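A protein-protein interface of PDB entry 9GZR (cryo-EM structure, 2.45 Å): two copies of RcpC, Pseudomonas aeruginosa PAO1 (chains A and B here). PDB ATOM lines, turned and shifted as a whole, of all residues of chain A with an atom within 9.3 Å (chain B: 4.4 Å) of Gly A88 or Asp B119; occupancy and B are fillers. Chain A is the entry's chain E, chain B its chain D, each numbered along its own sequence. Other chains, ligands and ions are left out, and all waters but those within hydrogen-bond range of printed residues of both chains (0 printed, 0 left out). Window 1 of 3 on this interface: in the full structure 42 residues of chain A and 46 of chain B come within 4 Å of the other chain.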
ATOM      1  N   GLU A  85      -8.569  -9.484 -17.609  1.00  0.00           N
ATOM      2  CA  GLU A  85      -8.989 -10.549 -18.510  1.00  0.00           C
ATOM      3  C   GLU A  85      -9.883  -9.995 -19.608  1.00  0.00           C
ATOM      4  O   GLU A  85     -10.914  -9.384 -19.308  1.00  0.00           O
ATOM      5  CB  GLU A  85      -9.729 -11.634 -17.745  1.00  0.00           C
ATOM      6  CG  GLU A  85     -10.216 -12.783 -18.607  1.00  0.00           C
ATOM      7  CD  GLU A  85     -10.781 -13.920 -17.785  1.00  0.00           C
ATOM      8  OE1 GLU A  85     -10.739 -13.832 -16.540  1.00  0.00           O
ATOM      9  OE2 GLU A  85     -11.266 -14.903 -18.381  1.00  0.00           O
ATOM     10  N   PRO A  86      -9.522 -10.173 -20.877  1.00  0.00           N
ATOM     11  CA  PRO A  86     -10.419  -9.760 -21.963  1.00  0.00           C
ATOM     12  C   PRO A  86     -11.686 -10.598 -21.968  1.00  0.00           C
ATOM     13  O   PRO A  86     -11.666 -11.782 -21.622  1.00  0.00           O
ATOM     14  CB  PRO A  86      -9.580 -10.002 -23.222  1.00  0.00           C
ATOM     15  CG  PRO A  86      -8.640 -11.081 -22.822  1.00  0.00           C
ATOM     16  CD  PRO A  86      -8.283 -10.771 -21.397  1.00  0.00           C
ATOM     17  N   GLY A  87     -12.785  -9.982 -22.358  1.00  0.00           N
ATOM     18  CA  GLY A  87     -14.039 -10.695 -22.482  1.00  0.00           C
ATOM     19  C   GLY A  87     -15.160  -9.937 -21.802  1.00  0.00           C
ATOM     20  O   GLY A  87     -14.949  -8.939 -21.121  1.00  0.00           O
ATOM     21  N   GLY A  88     -16.370 -10.449 -22.007  1.00  0.00           N
ATOM     22  CA  GLY A  88     -17.550  -9.910 -21.377  1.00  0.00           C
ATOM     23  C   GLY A  88     -18.356 -10.989 -20.685  1.00  0.00           C
ATOM     24  O   GLY A  88     -18.069 -12.184 -20.808  1.00  0.00           O
ATOM     25  N   PRO A  89     -19.381 -10.585 -19.930  1.00  0.00           N
ATOM     26  CA  PRO A  89     -20.189 -11.586 -19.215  1.00  0.00           C
ATOM     27  C   PRO A  89     -20.995 -12.493 -20.129  1.00  0.00           C
ATOM     28  O   PRO A  89     -21.140 -13.685 -19.828  1.00  0.00           O
ATOM     29  CB  PRO A  89     -21.090 -10.717 -18.329  1.00  0.00           C
ATOM     30  CG  PRO A  89     -21.183  -9.427 -19.065  1.00  0.00           C
ATOM     31  CD  PRO A  89     -19.809  -9.214 -19.613  1.00  0.00           C
ATOM     32  N   LEU A  90     -21.508 -11.970 -21.245  1.00  0.00           N
ATOM     33  CA  LEU A  90     -22.390 -12.754 -22.105  1.00  0.00           C
ATOM     34  C   LEU A  90     -21.711 -14.025 -22.599  1.00  0.00           C
ATOM     35  O   LEU A  90     -22.352 -15.075 -22.716  1.00  0.00           O
ATOM     36  CB  LEU A  90     -22.854 -11.911 -23.291  1.00  0.00           C
ATOM     37  CG  LEU A  90     -24.214 -11.227 -23.189  1.00  0.00           C
ATOM     38  CD1 LEU A  90     -24.621 -10.681 -24.540  1.00  0.00           C
ATOM     39  CD2 LEU A  90     -25.262 -12.187 -22.662  1.00  0.00           C
ATOM     40  N   ALA A  91     -20.415 -13.952 -22.894  1.00  0.00           N
ATOM     41  CA  ALA A  91     -19.684 -15.098 -23.414  1.00  0.00           C
ATOM     42  C   ALA A  91     -19.485 -16.198 -22.380  1.00  0.00           C
ATOM     43  O   ALA A  91     -19.063 -17.298 -22.750  1.00  0.00           O
ATOM     44  CB  ALA A  91     -18.325 -14.652 -23.956  1.00  0.00           C
ATOM     45  N   ARG A  92     -19.769 -15.936 -21.108  1.00  0.00           N
ATOM     46  CA  ARG A  92     -19.602 -16.936 -20.066  1.00  0.00           C
ATOM     47  C   ARG A  92     -20.868 -17.734 -19.789  1.00  0.00           C
ATOM     48  O   ARG A  92     -20.857 -18.588 -18.896  1.00  0.00           O
ATOM     49  CB  ARG A  92     -19.131 -16.267 -18.772  1.00  0.00           C
ATOM     50  CG  ARG A  92     -17.971 -15.315 -18.966  1.00  0.00           C
ATOM     51  CD  ARG A  92     -17.122 -15.218 -17.717  1.00  0.00           C
ATOM     52  NE  ARG A  92     -17.462 -14.044 -16.924  1.00  0.00           N
ATOM     53  CZ  ARG A  92     -17.884 -14.084 -15.668  1.00  0.00           C
ATOM     54  NH1 ARG A  92     -18.032 -15.232 -15.025  1.00  0.00           N
ATOM     55  NH2 ARG A  92     -18.166 -12.946 -15.041  1.00  0.00           N
ATOM     56  N   THR A  93     -21.947 -17.487 -20.527  1.00  0.00           N
ATOM     57  CA  THR A  93     -23.241 -18.096 -20.251  1.00  0.00           C
ATOM     58  C   THR A  93     -23.713 -19.026 -21.360  1.00  0.00           C
ATOM     59  O   THR A  93     -24.807 -19.587 -21.254  1.00  0.00           O
ATOM     60  CB  THR A  93     -24.294 -17.013 -20.009  1.00  0.00           C
ATOM     61  OG1 THR A  93     -24.617 -16.373 -21.250  1.00  0.00           O
ATOM     62  CG2 THR A  93     -23.778 -15.973 -19.032  1.00  0.00           C
ATOM     63  N   ILE A  94     -22.925 -19.211 -22.415  1.00  0.00           N
ATOM     64  CA  ILE A  94     -23.356 -20.047 -23.528  1.00  0.00           C
ATOM     65  C   ILE A  94     -22.358 -21.172 -23.762  1.00  0.00           C
ATOM     66  O   ILE A  94     -21.343 -21.275 -23.065  1.00  0.00           O
ATOM     67  CB  ILE A  94     -23.561 -19.218 -24.809  1.00  0.00           C
ATOM     68  CG1 ILE A  94     -22.410 -18.236 -25.008  1.00  0.00           C
ATOM     69  CG2 ILE A  94     -24.885 -18.481 -24.761  1.00  0.00           C
ATOM     70  CD1 ILE A  94     -22.225 -17.814 -26.443  1.00  0.00           C
ATOM     71  N   ALA A 100     -25.273 -15.754 -28.953  1.00  0.00           N
ATOM     72  CA  ALA A 100     -26.052 -14.795 -28.175  1.00  0.00           C
ATOM     73  C   ALA A 100     -26.415 -13.614 -29.067  1.00  0.00           C
ATOM     74  O   ALA A 100     -25.533 -12.874 -29.513  1.00  0.00           O
ATOM     75  CB  ALA A 100     -25.277 -14.335 -26.943  1.00  0.00           C
ATOM     76  N   ILE A 155     -29.335  -9.733 -15.592  1.00  0.00           N
ATOM     77  CA  ILE A 155     -28.465 -10.783 -16.105  1.00  0.00           C
ATOM     78  C   ILE A 155     -28.061 -11.686 -14.948  1.00  0.00           C
ATOM     79  O   ILE A 155     -27.845 -11.219 -13.826  1.00  0.00           O
ATOM     80  CB  ILE A 155     -27.230 -10.189 -16.818  1.00  0.00           C
ATOM     81  CG1 ILE A 155     -26.309 -11.294 -17.336  1.00  0.00           C
ATOM     82  CG2 ILE A 155     -26.479  -9.241 -15.899  1.00  0.00           C
ATOM     83  CD1 ILE A 155     -25.482 -10.886 -18.529  1.00  0.00           C
ATOM     84  N   VAL A 157     -25.171 -14.285 -14.345  1.00  0.00           N
ATOM     85  CA  VAL A 157     -23.924 -14.862 -14.831  1.00  0.00           C
ATOM     86  C   VAL A 157     -23.321 -15.802 -13.795  1.00  0.00           C
ATOM     87  O   VAL A 157     -22.650 -16.774 -14.143  1.00  0.00           O
ATOM     88  CB  VAL A 157     -22.923 -13.765 -15.209  1.00  0.00           C
ATOM     89  CG1 VAL A 157     -23.207 -13.252 -16.608  1.00  0.00           C
ATOM     90  CG2 VAL A 157     -22.986 -12.629 -14.203  1.00  0.00           C
ATOM     91  N   VAL B 115     -21.512  -6.159 -24.563  1.00  0.00           N
ATOM     92  CA  VAL B 115     -20.297  -6.523 -25.283  1.00  0.00           C
ATOM     93  C   VAL B 115     -19.142  -5.672 -24.771  1.00  0.00           C
ATOM     94  O   VAL B 115     -19.237  -4.441 -24.708  1.00  0.00           O
ATOM     95  CB  VAL B 115     -20.484  -6.352 -26.795  1.00  0.00           C
ATOM     96  CG1 VAL B 115     -19.192  -6.659 -27.524  1.00  0.00           C
ATOM     97  CG2 VAL B 115     -21.595  -7.248 -27.290  1.00  0.00           C
ATOM     98  N   LEU B 116     -18.050  -6.323 -24.403  1.00  0.00           N
ATOM     99  CA  LEU B 116     -16.848  -5.661 -23.938  1.00  0.00           C
ATOM    100  C   LEU B 116     -15.682  -5.968 -24.873  1.00  0.00           C
ATOM    101  O   LEU B 116     -15.711  -6.970 -25.593  1.00  0.00           O
ATOM    102  CB  LEU B 116     -16.491  -6.105 -22.515  1.00  0.00           C
ATOM    103  CG  LEU B 116     -17.136  -5.324 -21.371  1.00  0.00           C
ATOM    104  CD1 LEU B 116     -16.555  -5.757 -20.037  1.00  0.00           C
ATOM    105  CD2 LEU B 116     -16.978  -3.830 -21.568  1.00  0.00           C
ATOM    106  N   PRO B 117     -14.654  -5.118 -24.907  1.00  0.00           N
ATOM    107  CA  PRO B 117     -13.487  -5.410 -25.746  1.00  0.00           C
ATOM    108  C   PRO B 117     -12.842  -6.733 -25.361  1.00  0.00           C
ATOM    109  O   PRO B 117     -12.749  -7.084 -24.184  1.00  0.00           O
ATOM    110  CB  PRO B 117     -12.553  -4.229 -25.472  1.00  0.00           C
ATOM    111  CG  PRO B 117     -13.457  -3.137 -25.054  1.00  0.00           C
ATOM    112  CD  PRO B 117     -14.545  -3.795 -24.270  1.00  0.00           C
ATOM    113  N   GLY B 118     -12.392  -7.467 -26.374  1.00  0.00           N
ATOM    114  CA  GLY B 118     -11.852  -8.793 -26.201  1.00  0.00           C
ATOM    115  C   GLY B 118     -12.788  -9.914 -26.603  1.00  0.00           C
ATOM    116  O   GLY B 118     -12.342 -11.060 -26.717  1.00  0.00           O
ATOM    117  N   ASP B 119     -14.065  -9.616 -26.822  1.00  0.00           N
ATOM    118  CA  ASP B 119     -15.022 -10.622 -27.247  1.00  0.00           C
ATOM    119  C   ASP B 119     -14.817 -10.973 -28.715  1.00  0.00           C
ATOM    120  O   ASP B 119     -14.171 -10.245 -29.473  1.00  0.00           O
ATOM    121  CB  ASP B 119     -16.455 -10.132 -27.040  1.00  0.00           C
ATOM    122  CG  ASP B 119     -16.830 -10.022 -25.580  1.00  0.00           C
ATOM    123  OD1 ASP B 119     -15.929  -9.788 -24.754  1.00  0.00           O
ATOM    124  OD2 ASP B 119     -18.028 -10.157 -25.258  1.00  0.00           O
ATOM    125  N   TYR B 120     -15.377 -12.109 -29.112  1.00  0.00           N
ATOM    126  CA  TYR B 120     -15.391 -12.541 -30.500  1.00  0.00           C
ATOM    127  C   TYR B 120     -16.833 -12.652 -30.967  1.00  0.00           C
ATOM    128  O   TYR B 120     -17.675 -13.239 -30.280  1.00  0.00           O
ATOM    129  CB  TYR B 120     -14.671 -13.877 -30.679  1.00  0.00           C
ATOM    130  CG  TYR B 120     -13.167 -13.748 -30.707  1.00  0.00           C
ATOM    131  CD1 TYR B 120     -12.450 -13.519 -29.543  1.00  0.00           C
ATOM    132  CD2 TYR B 120     -12.466 -13.848 -31.897  1.00  0.00           C
ATOM    133  CE1 TYR B 120     -11.080 -13.397 -29.564  1.00  0.00           C
ATOM    134  CE2 TYR B 120     -11.098 -13.727 -31.928  1.00  0.00           C
ATOM    135  CZ  TYR B 120     -10.409 -13.503 -30.759  1.00  0.00           C
ATOM    136  OH  TYR B 120      -9.041 -13.382 -30.785  1.00  0.00           O
ATOM    137  N   VAL B 121     -17.116 -12.088 -32.138  1.00  0.00           N
ATOM    138  CA  VAL B 121     -18.479 -11.919 -32.616  1.00  0.00           C
ATOM    139  C   VAL B 121     -18.582 -12.400 -34.056  1.00  0.00           C
ATOM    140  O   VAL B 121     -17.590 -12.515 -34.777  1.00  0.00           O
ATOM    141  CB  VAL B 121     -18.955 -10.454 -32.515  1.00  0.00           C
ATOM    142  CG1 VAL B 121     -19.196 -10.067 -31.068  1.00  0.00           C
ATOM    143  CG2 VAL B 121     -17.946  -9.525 -33.158  1.00  0.00           C
ATOM    144  N   VAL B 146     -14.687 -12.358 -35.265  1.00  0.00           N
ATOM    145  CA  VAL B 146     -14.020 -11.066 -35.366  1.00  0.00           C
ATOM    146  C   VAL B 146     -13.827 -10.512 -33.963  1.00  0.00           C
ATOM    147  O   VAL B 146     -14.780 -10.452 -33.178  1.00  0.00           O
ATOM    148  CB  VAL B 146     -14.820 -10.081 -36.239  1.00  0.00           C
ATOM    149  CG1 VAL B 146     -14.447  -8.647 -35.912  1.00  0.00           C
ATOM    150  CG2 VAL B 146     -14.585 -10.366 -37.705  1.00  0.00           C
ATOM    151  N   ARG B 147     -12.597 -10.116 -33.646  1.00  0.00           N
ATOM    152  CA  ARG B 147     -12.305  -9.537 -32.345  1.00  0.00           C
ATOM    153  C   ARG B 147     -12.873  -8.126 -32.241  1.00  0.00           C
ATOM    154  O   ARG B 147     -13.041  -7.422 -33.240  1.00  0.00           O
ATOM    155  CB  ARG B 147     -10.798  -9.509 -32.097  1.00  0.00           C
ATOM    156  CG  ARG B 147     -10.403  -9.920 -30.691  1.00  0.00           C
ATOM    157  CD  ARG B 147      -9.153  -9.201 -30.211  1.00  0.00           C
ATOM    158  NE  ARG B 147      -8.110  -9.159 -31.229  1.00  0.00           N
ATOM    159  CZ  ARG B 147      -7.067  -8.341 -31.196  1.00  0.00           C
ATOM    160  NH1 ARG B 147      -6.888  -7.489 -30.201  1.00  0.00           N
ATOM    161  NH2 ARG B 147      -6.182  -8.378 -32.187  1.00  0.00           N
ATOM    162  N   VAL B 148     -13.165  -7.716 -31.013  1.00  0.00           N
ATOM    163  CA  VAL B 148     -13.723  -6.402 -30.721  1.00  0.00           C
ATOM    164  C   VAL B 148     -12.630  -5.580 -30.055  1.00  0.00           C
ATOM    165  O   VAL B 148     -12.079  -5.984 -29.024  1.00  0.00           O
ATOM    166  CB  VAL B 148     -14.970  -6.497 -29.831  1.00  0.00           C
ATOM    167  CG1 VAL B 148     -15.490  -5.113 -29.495  1.00  0.00           C
ATOM    168  CG2 VAL B 148     -16.047  -7.316 -30.517  1.00  0.00           C
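O of Pro B117 lies within hydrogen-bond range of N of Gly A87, at 3.4 Å. The side-chain carboxylate of Asp B119 lies within hydrogen-bond range of the backbone NH of Gly A88 (2.9 Å).
N of Gly B118 sits at hydrogen-bond distance from O of Val B148 (3.1 Å). N of Val B148 is in hydrogen-bond range of O of Asp B119, 3.1 Å away.
Among the printed residues, merely in contact across the chains: Gly A87 with Asp B119 (3.1 Å), Gly A87 with Leu B116 (3.5 Å) and Pro A86 with Gly B118 (3.9 Å).
Gly A88 touches just one residue of chain B: Asp B119. Asp B119 touches two residues of chain A. Gly B118 touches one residue of chain A. Of the printed residues of chain B, Pro A86 touches Gly B118. Of the printed residues of chain A, Leu B116 touches Gly A87. The nearest residue of chain B that does not touch Gly A88 is Leu B116 (4.1 Å).
Printed residues of chain A that touch a printed residue of chain B: Pro A86, Gly A87 and Gly A88. Of the 10 printed residues of chain B, 4 touch a printed residue of chain A. Among the printed residues, 5 pairs touch across the chains. Among the printed residues, no Asp or Glu carboxylate lies within 4 Å of a Lys or Arg side-chain nitrogen of the other chain.
No position is printed for both chains. Of the 5 pairs that touch across the chains among the printed residues, none has its exchanged pair printed and touching as well.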
